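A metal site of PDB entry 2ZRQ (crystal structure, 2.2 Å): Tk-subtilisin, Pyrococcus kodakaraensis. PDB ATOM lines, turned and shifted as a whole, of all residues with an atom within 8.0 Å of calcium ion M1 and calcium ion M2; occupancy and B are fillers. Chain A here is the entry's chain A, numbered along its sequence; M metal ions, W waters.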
ATOM      1  N   ALA A 142     -22.675 -22.063  -5.196  1.00  0.00           N
ATOM      2  CA  ALA A 142     -23.777 -23.035  -5.050  1.00  0.00           C
ATOM      3  C   ALA A 142     -23.650 -24.260  -5.963  1.00  0.00           C
ATOM      4  O   ALA A 142     -23.602 -25.413  -5.504  1.00  0.00           O
ATOM      5  CB  ALA A 142     -25.168 -22.366  -5.232  1.00  0.00           C
ATOM      6  N   ASP A 143     -23.544 -24.013  -7.259  1.00  0.00           N
ATOM      7  CA  ASP A 143     -23.597 -25.092  -8.227  1.00  0.00           C
ATOM      8  C   ASP A 143     -22.377 -24.944  -9.109  1.00  0.00           C
ATOM      9  O   ASP A 143     -22.480 -24.456 -10.239  1.00  0.00           O
ATOM     10  CB  ASP A 143     -24.894 -25.009  -9.034  1.00  0.00           C
ATOM     11  CG  ASP A 143     -25.008 -26.099 -10.094  1.00  0.00           C
ATOM     12  OD1 ASP A 143     -24.336 -27.138 -10.019  1.00  0.00           O
ATOM     13  OD2 ASP A 143     -25.810 -25.929 -11.016  1.00  0.00           O
ATOM     14  N   LYS A 144     -21.219 -25.365  -8.591  1.00  0.00           N
ATOM     15  CA  LYS A 144     -19.953 -25.087  -9.248  1.00  0.00           C
ATOM     16  C   LYS A 144     -19.816 -25.687 -10.658  1.00  0.00           C
ATOM     17  O   LYS A 144     -19.241 -25.053 -11.525  1.00  0.00           O
ATOM     18  CB  LYS A 144     -18.729 -25.339  -8.332  1.00  0.00           C
ATOM     19  CG  LYS A 144     -18.299 -26.799  -8.115  1.00  0.00           C
ATOM     20  CD  LYS A 144     -16.735 -26.888  -7.909  1.00  0.00           C
ATOM     21  CE  LYS A 144     -16.243 -28.339  -7.592  1.00  0.00           C
ATOM     22  NZ  LYS A 144     -16.538 -29.424  -8.648  1.00  0.00           N
ATOM     23  N   ASP A 145     -20.304 -26.905 -10.860  1.00  0.00           N
ATOM     24  CA  ASP A 145     -20.234 -27.555 -12.174  1.00  0.00           C
ATOM     25  C   ASP A 145     -21.475 -27.244 -13.071  1.00  0.00           C
ATOM     26  O   ASP A 145     -21.593 -27.780 -14.166  1.00  0.00           O
ATOM     27  CB  ASP A 145     -20.018 -29.080 -12.011  1.00  0.00           C
ATOM     28  CG  ASP A 145     -21.229 -29.791 -11.360  1.00  0.00           C
ATOM     29  OD1 ASP A 145     -21.332 -31.012 -11.534  1.00  0.00           O
ATOM     30  OD2 ASP A 145     -22.077 -29.132 -10.695  1.00  0.00           O
ATOM     31  N   GLY A 146     -22.388 -26.367 -12.642  1.00  0.00           N
ATOM     32  CA  GLY A 146     -23.516 -25.972 -13.505  1.00  0.00           C
ATOM     33  C   GLY A 146     -24.450 -27.079 -14.009  1.00  0.00           C
ATOM     34  O   GLY A 146     -25.093 -26.876 -15.060  1.00  0.00           O
ATOM     35  N   ASP A 147     -24.585 -28.200 -13.262  1.00  0.00           N
ATOM     36  CA  ASP A 147     -25.507 -29.315 -13.663  1.00  0.00           C
ATOM     37  C   ASP A 147     -26.921 -29.199 -13.092  1.00  0.00           C
ATOM     38  O   ASP A 147     -27.742 -30.100 -13.288  1.00  0.00           O
ATOM     39  CB  ASP A 147     -24.940 -30.699 -13.329  1.00  0.00           C
ATOM     40  CG  ASP A 147     -24.868 -30.973 -11.834  1.00  0.00           C
ATOM     41  OD1 ASP A 147     -25.175 -30.066 -11.037  1.00  0.00           O
ATOM     42  OD2 ASP A 147     -24.522 -32.106 -11.438  1.00  0.00           O
ATOM     43  N   GLY A 148     -27.197 -28.095 -12.396  1.00  0.00           N
ATOM     44  CA  GLY A 148     -28.474 -27.839 -11.739  1.00  0.00           C
ATOM     45  C   GLY A 148     -28.742 -28.573 -10.426  1.00  0.00           C
ATOM     46  O   GLY A 148     -29.809 -28.472  -9.853  1.00  0.00           O
ATOM     47  N   ILE A 149     -27.777 -29.366  -9.958  1.00  0.00           N
ATOM     48  CA  ILE A 149     -27.936 -30.151  -8.730  1.00  0.00           C
ATOM     49  C   ILE A 149     -26.981 -29.595  -7.640  1.00  0.00           C
ATOM     50  O   ILE A 149     -25.836 -29.324  -7.925  1.00  0.00           O
ATOM     51  CB  ILE A 149     -27.695 -31.672  -8.977  1.00  0.00           C
ATOM     52  CG1 ILE A 149     -28.626 -32.188 -10.084  1.00  0.00           C
ATOM     53  CG2 ILE A 149     -27.967 -32.455  -7.701  1.00  0.00           C
ATOM     54  CD1 ILE A 149     -28.292 -33.606 -10.619  1.00  0.00           C
ATOM     55  N   ILE A 150     -27.468 -29.429  -6.425  1.00  0.00           N
ATOM     56  CA  ILE A 150     -26.681 -28.853  -5.326  1.00  0.00           C
ATOM     57  C   ILE A 150     -26.554 -29.880  -4.176  1.00  0.00           C
ATOM     58  O   ILE A 150     -25.476 -30.437  -3.972  1.00  0.00           O
ATOM     59  CB  ILE A 150     -27.315 -27.496  -4.858  1.00  0.00           C
ATOM     60  CG1 ILE A 150     -27.140 -26.425  -5.936  1.00  0.00           C
ATOM     61  CG2 ILE A 150     -26.719 -27.006  -3.597  1.00  0.00           C
ATOM     62  CD1 ILE A 150     -28.203 -25.317  -5.922  1.00  0.00           C
ATOM     63  N   ALA A 151     -27.644 -30.138  -3.440  1.00  0.00           N
ATOM     64  CA  ALA A 151     -27.667 -31.216  -2.442  1.00  0.00           C
ATOM     65  C   ALA A 151     -27.533 -32.573  -3.156  1.00  0.00           C
ATOM     66  O   ALA A 151     -28.221 -32.806  -4.146  1.00  0.00           O
ATOM     67  CB  ALA A 151     -28.968 -31.189  -1.652  1.00  0.00           C
ATOM     68  N   GLY A 152     -26.688 -33.455  -2.661  1.00  0.00           N
ATOM     69  CA  GLY A 152     -26.577 -34.798  -3.224  1.00  0.00           C
ATOM     70  C   GLY A 152     -25.671 -34.834  -4.448  1.00  0.00           C
ATOM     71  O   GLY A 152     -25.577 -35.888  -5.116  1.00  0.00           O
ATOM     72  N   ASP A 153     -25.019 -33.707  -4.755  1.00  0.00           N
ATOM     73  CA  ASP A 153     -24.038 -33.628  -5.873  1.00  0.00           C
ATOM     74  C   ASP A 153     -22.601 -33.643  -5.363  1.00  0.00           C
ATOM     75  O   ASP A 153     -22.190 -32.693  -4.706  1.00  0.00           O
ATOM     76  CB  ASP A 153     -24.263 -32.379  -6.721  1.00  0.00           C
ATOM     77  CG  ASP A 153     -23.368 -32.326  -7.947  1.00  0.00           C
ATOM     78  OD1 ASP A 153     -23.430 -31.327  -8.702  1.00  0.00           O
ATOM     79  OD2 ASP A 153     -22.585 -33.279  -8.187  1.00  0.00           O
ATOM     80  N   PRO A 154     -21.822 -34.736  -5.640  1.00  0.00           N
ATOM     81  CA  PRO A 154     -20.468 -34.870  -5.131  1.00  0.00           C
ATOM     82  C   PRO A 154     -19.494 -33.840  -5.729  1.00  0.00           C
ATOM     83  O   PRO A 154     -18.437 -33.610  -5.134  1.00  0.00           O
ATOM     84  CB  PRO A 154     -20.098 -36.319  -5.485  1.00  0.00           C
ATOM     85  CG  PRO A 154     -20.902 -36.620  -6.651  1.00  0.00           C
ATOM     86  CD  PRO A 154     -22.224 -35.933  -6.390  1.00  0.00           C
ATOM     87  N   ASP A 155     -19.902 -33.198  -6.822  1.00  0.00           N
ATOM     88  CA  ASP A 155     -19.149 -32.078  -7.422  1.00  0.00           C
ATOM     89  C   ASP A 155     -19.418 -30.737  -6.709  1.00  0.00           C
ATOM     90  O   ASP A 155     -18.749 -29.755  -6.978  1.00  0.00           O
ATOM     91  CB  ASP A 155     -19.440 -31.970  -8.942  1.00  0.00           C
ATOM     92  CG  ASP A 155     -19.193 -33.301  -9.673  1.00  0.00           C
ATOM     93  OD1 ASP A 155     -18.033 -33.830  -9.604  1.00  0.00           O
ATOM     94  OD2 ASP A 155     -20.148 -33.847 -10.264  1.00  0.00           O
ATOM     95  N   ASP A 156     -20.407 -30.695  -5.824  1.00  0.00           N
ATOM     96  CA  ASP A 156     -20.602 -29.518  -4.962  1.00  0.00           C
ATOM     97  C   ASP A 156     -20.347 -29.838  -3.505  1.00  0.00           C
ATOM     98  O   ASP A 156     -20.160 -30.995  -3.145  1.00  0.00           O
ATOM     99  CB  ASP A 156     -21.965 -28.903  -5.193  1.00  0.00           C
ATOM    100  CG  ASP A 156     -21.997 -28.116  -6.461  1.00  0.00           C
ATOM    101  OD1 ASP A 156     -21.280 -27.095  -6.546  1.00  0.00           O
ATOM    102  OD2 ASP A 156     -22.715 -28.533  -7.387  1.00  0.00           O
ATOM    103  N   ASP A 157     -20.333 -28.801  -2.658  1.00  0.00           N
ATOM    104  CA  ASP A 157     -20.098 -29.017  -1.230  1.00  0.00           C
ATOM    105  C   ASP A 157     -21.237 -28.430  -0.339  1.00  0.00           C
ATOM    106  O   ASP A 157     -21.020 -28.143   0.835  1.00  0.00           O
ATOM    107  CB  ASP A 157     -18.722 -28.468  -0.839  1.00  0.00           C
ATOM    108  CG  ASP A 157     -18.588 -26.967  -1.088  1.00  0.00           C
ATOM    109  OD1 ASP A 157     -17.481 -26.443  -0.994  1.00  0.00           O
ATOM    110  OD2 ASP A 157     -19.615 -26.310  -1.383  1.00  0.00           O
HETATM  111 CA    CA M   1     -23.859 -29.271  -9.150  1.00  0.00          CA
HETATM  112 CA    CA M   2     -22.505 -32.958 -10.642  1.00  0.00          CA
HETATM  113  O   HOH W   1     -23.367 -35.158 -10.443  1.00  0.00           O
HETATM  114  O   HOH W   2     -22.080 -34.394 -12.752  1.00  0.00           O
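The side-chain carboxylate (OD1) of Asp 156 is in hydrogen-bond range of the backbone NH (N) of Lys 144 (2.7 Å). N of Gly 146 sits close to OD1 of Asp 143 (3.4 Å). The side-chain carboxylate (OD2) of Asp 143 lies within hydrogen-bond range of the backbone NH (N) of Gly 148, at 2.9 Å. O of Asp 155 sits at hydrogen-bond distance from NZ of Lys 144 (2.8 Å).
Along chain A the residues within 4 Å of calcium ion M1 span positions 143 to 156. The nearest printed residue that does not touch calcium ion M1 is Ile 150 (4.5 Å).
Of the 16 residues printed, 4 come within 4 Å of calcium ion M2. The nearest printed residue that does not touch calcium ion M2 is Pro 154 (5.2 Å).
Calcium ion M1 is bound by OD1 of Asp 153, OD2 of Asp 156, O of Ile 149, OD1 of Asp 143, OD2 of Asp 145 and OD1 of Asp 147. Calcium ion M1 has six donor atoms within binding distance.
The side-chain carboxylate (OD2) of Asp 147 is bound to calcium ion M2 (2.3 Å). Water W1 is bound to calcium ion M2 (2.4 Å). The side-chain carboxylate (OD1) of Asp 145 is bound to calcium ion M2 (2.4 Å). Calcium ion M2 is bound by OD2 of Asp 153 (2.5 Å). The side-chain carboxylate (OD2) of Asp 155 binds calcium ion M2 (2.5 Å). Calcium ion M2 is bound by water W2. The side-chain carboxylate (OD1) of Asp 153 binds calcium ion M2 (2.7 Å).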
